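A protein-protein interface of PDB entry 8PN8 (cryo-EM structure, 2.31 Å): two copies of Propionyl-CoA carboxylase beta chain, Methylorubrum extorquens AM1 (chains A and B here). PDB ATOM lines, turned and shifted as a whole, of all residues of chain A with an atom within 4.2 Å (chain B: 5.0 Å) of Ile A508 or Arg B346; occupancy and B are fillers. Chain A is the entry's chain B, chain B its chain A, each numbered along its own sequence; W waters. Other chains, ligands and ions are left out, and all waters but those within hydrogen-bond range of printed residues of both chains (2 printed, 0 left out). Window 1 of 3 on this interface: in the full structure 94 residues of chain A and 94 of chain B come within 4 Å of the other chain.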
ATOM      1  N   LYS A 381      12.484  32.132  17.426  1.00  0.00           N
ATOM      2  CA  LYS A 381      13.147  30.996  16.791  1.00  0.00           C
ATOM      3  C   LYS A 381      14.490  30.703  17.451  1.00  0.00           C
ATOM      4  O   LYS A 381      14.797  29.551  17.779  1.00  0.00           O
ATOM      5  CB  LYS A 381      13.333  31.261  15.298  1.00  0.00           C
ATOM      6  CG  LYS A 381      12.053  31.202  14.492  1.00  0.00           C
ATOM      7  CD  LYS A 381      12.301  31.570  13.043  1.00  0.00           C
ATOM      8  CE  LYS A 381      10.998  31.670  12.277  1.00  0.00           C
ATOM      9  NZ  LYS A 381      11.223  31.976  10.842  1.00  0.00           N
ATOM     10  N   PHE A 384      13.873  29.436  20.978  1.00  0.00           N
ATOM     11  CA  PHE A 384      13.435  28.048  20.913  1.00  0.00           C
ATOM     12  C   PHE A 384      14.603  27.112  20.648  1.00  0.00           C
ATOM     13  O   PHE A 384      14.720  26.059  21.285  1.00  0.00           O
ATOM     14  CB  PHE A 384      12.381  27.915  19.812  1.00  0.00           C
ATOM     15  CG  PHE A 384      11.481  26.725  19.952  1.00  0.00           C
ATOM     16  CD1 PHE A 384      11.933  25.453  19.649  1.00  0.00           C
ATOM     17  CD2 PHE A 384      10.168  26.885  20.354  1.00  0.00           C
ATOM     18  CE1 PHE A 384      11.101  24.365  19.769  1.00  0.00           C
ATOM     19  CE2 PHE A 384       9.331  25.799  20.472  1.00  0.00           C
ATOM     20  CZ  PHE A 384       9.799  24.538  20.179  1.00  0.00           C
ATOM     21  N   HIS A 505       7.377  15.918  17.040  1.00  0.00           N
ATOM     22  CA  HIS A 505       8.295  17.023  16.803  1.00  0.00           C
ATOM     23  C   HIS A 505       7.739  18.233  17.538  1.00  0.00           C
ATOM     24  O   HIS A 505       6.582  18.243  17.967  1.00  0.00           O
ATOM     25  CB  HIS A 505       8.483  17.315  15.310  1.00  0.00           C
ATOM     26  CG  HIS A 505       7.213  17.632  14.586  1.00  0.00           C
ATOM     27  ND1 HIS A 505       6.535  18.819  14.755  1.00  0.00           N
ATOM     28  CD2 HIS A 505       6.499  16.916  13.686  1.00  0.00           C
ATOM     29  CE1 HIS A 505       5.457  18.820  13.992  1.00  0.00           C
ATOM     30  NE2 HIS A 505       5.412  17.677  13.333  1.00  0.00           N
ATOM     31  N   ASP A 506       8.577  19.252  17.681  1.00  0.00           N
ATOM     32  CA  ASP A 506       8.163  20.481  18.334  1.00  0.00           C
ATOM     33  C   ASP A 506       7.365  21.349  17.363  1.00  0.00           C
ATOM     34  O   ASP A 506       7.162  21.003  16.196  1.00  0.00           O
ATOM     35  CB  ASP A 506       9.380  21.224  18.876  1.00  0.00           C
ATOM     36  CG  ASP A 506      10.437  21.456  17.816  1.00  0.00           C
ATOM     37  OD1 ASP A 506      10.256  22.363  16.980  1.00  0.00           O
ATOM     38  OD2 ASP A 506      11.448  20.726  17.814  1.00  0.00           O
ATOM     39  N   ASN A 507       6.903  22.497  17.852  1.00  0.00           N
ATOM     40  CA  ASN A 507       6.129  23.418  17.032  1.00  0.00           C
ATOM     41  C   ASN A 507       6.826  24.769  16.960  1.00  0.00           C
ATOM     42  O   ASN A 507       6.201  25.810  17.182  1.00  0.00           O
ATOM     43  CB  ASN A 507       4.708  23.568  17.577  1.00  0.00           C
ATOM     44  CG  ASN A 507       3.754  24.167  16.561  1.00  0.00           C
ATOM     45  OD1 ASN A 507       4.001  24.120  15.359  1.00  0.00           O
ATOM     46  ND2 ASN A 507       2.658  24.738  17.042  1.00  0.00           N
ATOM     47  N   ILE A 508       8.127  24.753  16.680  1.00  0.00           N
ATOM     48  CA  ILE A 508       8.897  25.998  16.587  1.00  0.00           C
ATOM     49  C   ILE A 508       8.274  26.894  15.524  1.00  0.00           C
ATOM     50  O   ILE A 508       7.876  26.396  14.451  1.00  0.00           O
ATOM     51  CB  ILE A 508      10.374  25.695  16.270  1.00  0.00           C
ATOM     52  CG1 ILE A 508      11.196  26.981  16.177  1.00  0.00           C
ATOM     53  CG2 ILE A 508      10.506  24.882  14.989  1.00  0.00           C
ATOM     54  CD1 ILE A 508      12.669  26.745  15.953  1.00  0.00           C
ATOM     55  N   PRO A 509       8.121  28.196  15.768  1.00  0.00           N
ATOM     56  CA  PRO A 509       7.499  29.062  14.762  1.00  0.00           C
ATOM     57  C   PRO A 509       8.319  29.121  13.483  1.00  0.00           C
ATOM     58  O   PRO A 509       9.547  29.023  13.497  1.00  0.00           O
ATOM     59  CB  PRO A 509       7.440  30.430  15.456  1.00  0.00           C
ATOM     60  CG  PRO A 509       8.435  30.345  16.564  1.00  0.00           C
ATOM     61  CD  PRO A 509       8.412  28.924  17.014  1.00  0.00           C
ATOM     62  N   LEU A 510       7.618  29.277  12.366  1.00  0.00           N
ATOM     63  CA  LEU A 510       8.257  29.308  11.058  1.00  0.00           C
ATOM     64  C   LEU A 510       8.090  30.673  10.395  1.00  0.00           C
ATOM     65  O   LEU A 510       7.203  31.448  10.753  1.00  0.00           O
ATOM     66  CB  LEU A 510       7.681  28.210  10.161  1.00  0.00           C
ATOM     67  CG  LEU A 510       7.796  26.786  10.705  1.00  0.00           C
ATOM     68  CD1 LEU A 510       7.080  25.806   9.797  1.00  0.00           C
ATOM     69  CD2 LEU A 510       9.254  26.398  10.867  1.00  0.00           C
ATOM     70  OXT LEU A 510       8.837  31.033   9.487  1.00  0.00           O
ATOM     71  N   SER B 154       6.221  22.457  23.982  1.00  0.00           N
ATOM     72  CA  SER B 154       5.842  22.586  22.582  1.00  0.00           C
ATOM     73  C   SER B 154       5.753  21.216  21.922  1.00  0.00           C
ATOM     74  O   SER B 154       6.683  20.410  22.007  1.00  0.00           O
ATOM     75  CB  SER B 154       6.847  23.465  21.844  1.00  0.00           C
ATOM     76  OG  SER B 154       6.508  23.584  20.476  1.00  0.00           O
ATOM     77  N   ALA B 341       0.730  27.903   6.039  1.00  0.00           N
ATOM     78  CA  ALA B 341       0.313  26.520   5.862  1.00  0.00           C
ATOM     79  C   ALA B 341       1.293  25.556   6.515  1.00  0.00           C
ATOM     80  O   ALA B 341       0.886  24.526   7.057  1.00  0.00           O
ATOM     81  CB  ALA B 341       0.155  26.208   4.376  1.00  0.00           C
ATOM     82  N   ALA B 342       2.592  25.869   6.472  1.00  0.00           N
ATOM     83  CA  ALA B 342       3.583  25.000   7.092  1.00  0.00           C
ATOM     84  C   ALA B 342       3.396  24.936   8.599  1.00  0.00           C
ATOM     85  O   ALA B 342       3.441  23.853   9.190  1.00  0.00           O
ATOM     86  CB  ALA B 342       4.990  25.482   6.747  1.00  0.00           C
ATOM     87  N   ARG B 343       3.182  26.088   9.240  1.00  0.00           N
ATOM     88  CA  ARG B 343       2.945  26.085  10.680  1.00  0.00           C
ATOM     89  C   ARG B 343       1.678  25.313  11.021  1.00  0.00           C
ATOM     90  O   ARG B 343       1.658  24.528  11.980  1.00  0.00           O
ATOM     91  CB  ARG B 343       2.860  27.517  11.204  1.00  0.00           C
ATOM     92  CG  ARG B 343       2.811  27.622  12.719  1.00  0.00           C
ATOM     93  CD  ARG B 343       4.193  27.480  13.328  1.00  0.00           C
ATOM     94  NE  ARG B 343       4.147  27.297  14.774  1.00  0.00           N
ATOM     95  CZ  ARG B 343       3.993  28.278  15.653  1.00  0.00           C
ATOM     96  NH1 ARG B 343       3.830  29.532  15.268  1.00  0.00           N
ATOM     97  NH2 ARG B 343       4.003  27.993  16.951  1.00  0.00           N
ATOM     98  N   PHE B 344       0.612  25.510  10.239  1.00  0.00           N
ATOM     99  CA  PHE B 344      -0.630  24.792  10.510  1.00  0.00           C
ATOM    100  C   PHE B 344      -0.449  23.283  10.355  1.00  0.00           C
ATOM    101  O   PHE B 344      -0.935  22.504  11.183  1.00  0.00           O
ATOM    102  CB  PHE B 344      -1.740  25.297   9.591  1.00  0.00           C
ATOM    103  CG  PHE B 344      -3.083  24.703   9.889  1.00  0.00           C
ATOM    104  CD1 PHE B 344      -3.826  25.150  10.965  1.00  0.00           C
ATOM    105  CD2 PHE B 344      -3.602  23.699   9.093  1.00  0.00           C
ATOM    106  CE1 PHE B 344      -5.059  24.607  11.244  1.00  0.00           C
ATOM    107  CE2 PHE B 344      -4.835  23.153   9.368  1.00  0.00           C
ATOM    108  CZ  PHE B 344      -5.564  23.607  10.445  1.00  0.00           C
ATOM    109  N   VAL B 345       0.249  22.855   9.303  1.00  0.00           N
ATOM    110  CA  VAL B 345       0.451  21.430   9.064  1.00  0.00           C
ATOM    111  C   VAL B 345       1.331  20.824  10.149  1.00  0.00           C
ATOM    112  O   VAL B 345       1.090  19.701  10.604  1.00  0.00           O
ATOM    113  CB  VAL B 345       1.036  21.206   7.656  1.00  0.00           C
ATOM    114  CG1 VAL B 345       1.537  19.782   7.498  1.00  0.00           C
ATOM    115  CG2 VAL B 345      -0.009  21.512   6.598  1.00  0.00           C
ATOM    116  N   ARG B 346       2.359  21.555  10.586  1.00  0.00           N
ATOM    117  CA  ARG B 346       3.200  21.068  11.674  1.00  0.00           C
ATOM    118  C   ARG B 346       2.397  20.900  12.957  1.00  0.00           C
ATOM    119  O   ARG B 346       2.549  19.896  13.663  1.00  0.00           O
ATOM    120  CB  ARG B 346       4.373  22.021  11.896  1.00  0.00           C
ATOM    121  CG  ARG B 346       5.408  22.004  10.785  1.00  0.00           C
ATOM    122  CD  ARG B 346       6.584  21.114  11.126  1.00  0.00           C
ATOM    123  NE  ARG B 346       7.346  21.638  12.252  1.00  0.00           N
ATOM    124  CZ  ARG B 346       8.498  21.137  12.672  1.00  0.00           C
ATOM    125  NH1 ARG B 346       9.058  20.098  12.078  1.00  0.00           N
ATOM    126  NH2 ARG B 346       9.104  21.694  13.716  1.00  0.00           N
ATOM    127  N   PHE B 347       1.529  21.865  13.273  1.00  0.00           N
ATOM    128  CA  PHE B 347       0.695  21.720  14.463  1.00  0.00           C
ATOM    129  C   PHE B 347      -0.240  20.524  14.342  1.00  0.00           C
ATOM    130  O   PHE B 347      -0.394  19.750  15.293  1.00  0.00           O
ATOM    131  CB  PHE B 347      -0.116  22.988  14.720  1.00  0.00           C
ATOM    132  CG  PHE B 347      -1.073  22.857  15.871  1.00  0.00           C
ATOM    133  CD1 PHE B 347      -0.643  23.055  17.169  1.00  0.00           C
ATOM    134  CD2 PHE B 347      -2.398  22.511  15.657  1.00  0.00           C
ATOM    135  CE1 PHE B 347      -1.515  22.924  18.228  1.00  0.00           C
ATOM    136  CE2 PHE B 347      -3.271  22.375  16.715  1.00  0.00           C
ATOM    137  CZ  PHE B 347      -2.828  22.582  18.001  1.00  0.00           C
ATOM    138  N   CYS B 348      -0.880  20.358  13.183  1.00  0.00           N
ATOM    139  CA  CYS B 348      -1.824  19.256  13.019  1.00  0.00           C
ATOM    140  C   CYS B 348      -1.125  17.907  13.109  1.00  0.00           C
ATOM    141  O   CYS B 348      -1.661  16.961  13.697  1.00  0.00           O
ATOM    142  CB  CYS B 348      -2.571  19.391  11.693  1.00  0.00           C
ATOM    143  SG  CYS B 348      -3.824  20.684  11.683  1.00  0.00           S
ATOM    144  N   ASN B 349       0.071  17.795  12.530  1.00  0.00           N
ATOM    145  CA  ASN B 349       0.806  16.537  12.604  1.00  0.00           C
ATOM    146  C   ASN B 349       1.298  16.263  14.019  1.00  0.00           C
ATOM    147  O   ASN B 349       1.303  15.111  14.464  1.00  0.00           O
ATOM    148  CB  ASN B 349       1.976  16.553  11.622  1.00  0.00           C
ATOM    149  CG  ASN B 349       2.763  15.262  11.637  1.00  0.00           C
ATOM    150  OD1 ASN B 349       2.260  14.213  11.243  1.00  0.00           O
ATOM    151  ND2 ASN B 349       4.008  15.333  12.084  1.00  0.00           N
ATOM    152  N   ALA B 350       1.718  17.306  14.740  1.00  0.00           N
ATOM    153  CA  ALA B 350       2.243  17.105  16.086  1.00  0.00           C
ATOM    154  C   ALA B 350       1.192  16.538  17.030  1.00  0.00           C
ATOM    155  O   ALA B 350       1.532  15.819  17.976  1.00  0.00           O
ATOM    156  CB  ALA B 350       2.794  18.420  16.637  1.00  0.00           C
ATOM    157  N   PHE B 384       8.477  20.586   3.513  1.00  0.00           N
ATOM    158  CA  PHE B 384       9.047  19.860   4.641  1.00  0.00           C
ATOM    159  C   PHE B 384       7.960  19.404   5.602  1.00  0.00           C
ATOM    160  O   PHE B 384       7.965  18.256   6.059  1.00  0.00           O
ATOM    161  CB  PHE B 384      10.057  20.757   5.360  1.00  0.00           C
ATOM    162  CG  PHE B 384      11.071  20.014   6.175  1.00  0.00           C
ATOM    163  CD1 PHE B 384      10.729  19.445   7.389  1.00  0.00           C
ATOM    164  CD2 PHE B 384      12.380  19.911   5.741  1.00  0.00           C
ATOM    165  CE1 PHE B 384      11.664  18.771   8.139  1.00  0.00           C
ATOM    166  CE2 PHE B 384      13.320  19.240   6.489  1.00  0.00           C
ATOM    167  CZ  PHE B 384      12.961  18.669   7.690  1.00  0.00           C
ATOM    168  N   ALA B 385       7.014  20.292   5.912  1.00  0.00           N
ATOM    169  CA  ALA B 385       5.932  19.938   6.823  1.00  0.00           C
ATOM    170  C   ALA B 385       5.076  18.816   6.252  1.00  0.00           C
ATOM    171  O   ALA B 385       4.691  17.890   6.975  1.00  0.00           O
ATOM    172  CB  ALA B 385       5.078  21.167   7.126  1.00  0.00           C
ATOM    173  N   GLN B 388       7.040  15.506   6.172  1.00  0.00           N
ATOM    174  CA  GLN B 388       7.296  15.030   7.522  1.00  0.00           C
ATOM    175  C   GLN B 388       6.053  14.456   8.188  1.00  0.00           C
ATOM    176  O   GLN B 388       6.173  13.733   9.181  1.00  0.00           O
ATOM    177  CB  GLN B 388       7.857  16.180   8.361  1.00  0.00           C
ATOM    178  CG  GLN B 388       8.454  15.785   9.688  1.00  0.00           C
ATOM    179  CD  GLN B 388       8.822  16.987  10.526  1.00  0.00           C
ATOM    180  OE1 GLN B 388       8.427  18.111  10.221  1.00  0.00           O
ATOM    181  NE2 GLN B 388       9.583  16.759  11.587  1.00  0.00           N
ATOM    182  N   ASP B 506      14.325  17.395  13.340  1.00  0.00           N
ATOM    183  CA  ASP B 506      14.684  17.663  11.960  1.00  0.00           C
ATOM    184  C   ASP B 506      15.423  18.996  11.861  1.00  0.00           C
ATOM    185  O   ASP B 506      15.622  19.707  12.850  1.00  0.00           O
ATOM    186  CB  ASP B 506      13.436  17.651  11.082  1.00  0.00           C
ATOM    187  CG  ASP B 506      12.348  18.561  11.611  1.00  0.00           C
ATOM    188  OD1 ASP B 506      12.454  19.789  11.425  1.00  0.00           O
ATOM    189  OD2 ASP B 506      11.388  18.049  12.221  1.00  0.00           O
ATOM    190  N   ILE B 508      14.464  21.575   9.639  1.00  0.00           N
ATOM    191  CA  ILE B 508      13.612  22.361   8.740  1.00  0.00           C
ATOM    192  C   ILE B 508      14.146  23.785   8.659  1.00  0.00           C
ATOM    193  O   ILE B 508      14.552  24.353   9.694  1.00  0.00           O
ATOM    194  CB  ILE B 508      12.150  22.338   9.225  1.00  0.00           C
ATOM    195  CG1 ILE B 508      11.238  23.119   8.277  1.00  0.00           C
ATOM    196  CG2 ILE B 508      12.032  22.874  10.646  1.00  0.00           C
ATOM    197  CD1 ILE B 508       9.780  23.068   8.663  1.00  0.00           C
ATOM    198  N   LEU B 510      14.541  27.772   8.691  1.00  0.00           N
ATOM    199  CA  LEU B 510      13.860  28.780   9.491  1.00  0.00           C
ATOM    200  C   LEU B 510      13.912  30.147   8.816  1.00  0.00           C
ATOM    201  O   LEU B 510      14.763  30.401   7.963  1.00  0.00           O
ATOM    202  CB  LEU B 510      14.479  28.854  10.888  1.00  0.00           C
ATOM    203  CG  LEU B 510      14.472  27.548  11.682  1.00  0.00           C
ATOM    204  CD1 LEU B 510      15.222  27.711  12.989  1.00  0.00           C
ATOM    205  CD2 LEU B 510      13.049  27.088  11.935  1.00  0.00           C
ATOM    206  OXT LEU B 510      13.104  31.028   9.103  1.00  0.00           O
HETATM  207  O   HOH W   1      11.426  19.956  14.744  1.00  0.00           O
HETATM  208  O   HOH W   2       6.426  24.518  13.629  1.00  0.00           O
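NH1 of Arg B346 lies within hydrogen-bond range of OE1 of Gln B388 (2.8 Å). NH1 of Arg B346 lies within salt-bridge range of OD2 of Asp B506 (3.1 Å). NZ of Lys A381 lies within salt-bridge range of OXT of Leu A510, at 2.9 Å. The side-chain carboxylate (OD1) of Asp A506 lies within hydrogen-bond range of the backbone NH (N) of Ile A508, at 3.2 Å.
OG of Ser B154 sits at hydrogen-bond distance from N of Asn A507 (2.9 Å). The guanidinium group (NH2) of Arg B343 lies within hydrogen-bond range of the backbone carbonyl oxygen (O) of Asn A507. The guanidinium group of Arg B346 lies within salt-bridge range of the side-chain carboxylate of Asp A506 (3.5 Å). A ring nitrogen (NE2) of His A505 lies within hydrogen-bond range of the side-chain amide nitrogen of Asn B349 (3.0 Å). The chain-end carboxylate (OXT) of Leu B510 lies within salt-bridge range of the side-chain amino group (NZ) of Lys A381, 2.7 Å away.
Positions printed for both chains: 384, 506, 508 and 510. Of the 16 pairs that touch across the chains among the printed residues, none has its exchanged pair printed and touching as well.
Water W2 lies within hydrogen-bond range of O of Ile A508 (2.5 Å), OD1 of Asn A507 (3.0 Å) and NE of Arg B346 (3.3 Å). Water W1 lies within hydrogen-bond range of NH2 of Arg B346 (3.1 Å), OD2 of Asp B506 (3.2 Å) and OD2 of Asp A506 (3.2 Å).
Phe A384 touches Ser B154. CE1 of His A505 touches O of Arg B346, 3.1 Å away. His A505 touches Gln B388. OG of Ser B154 touches C of Asp A506, at 3.9 Å. ND2 of Asn A507 touches CD1 of Phe B347, 3.7 Å away. Ile A508 touches Arg B343 (O to NE, 3.8 Å). Arg B346 touches Ile A508. CZ of Arg B343 touches CA of Pro A509, at 3.7 Å. Ala B342 touches Leu A510 (CB to CD1, 3.7 Å). Leu A510 touches Arg B343 (CD1 to N, 3.9 Å).
Ile A508 touches just these residues of chain B: Arg B343 and Arg B346. Of the printed residues of chain B, Leu A510 touches Ala B342 and Arg B343. Arg B346 touches just these residues of chain A: His A505, Asp A506 and Ile A508. Printed residues of chain A within 4 Å of Phe B347: Asn A507. Printed residues of chain A within 4 Å of Asn B349: His A505 (3.0 Å). Of the printed residues of chain A, Leu B510 touches Lys A381. The nearest residue of chain A that does not touch Arg B346 is Asn A507 (4.1 Å). The nearest printed residue of chain A that does not touch Gln B388 is Asp A506 (6.7 Å).
Of the 8 printed residues of chain A, 8 touch a printed residue of chain B. Hydrophobic or aromatic side chains of chain A within 4 Å of the printed part of chain B: Phe A384, His A505, Ile A508, Pro A509 and Leu A510. Of the 17 printed residues of chain B, 9 touch a printed residue of chain A.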
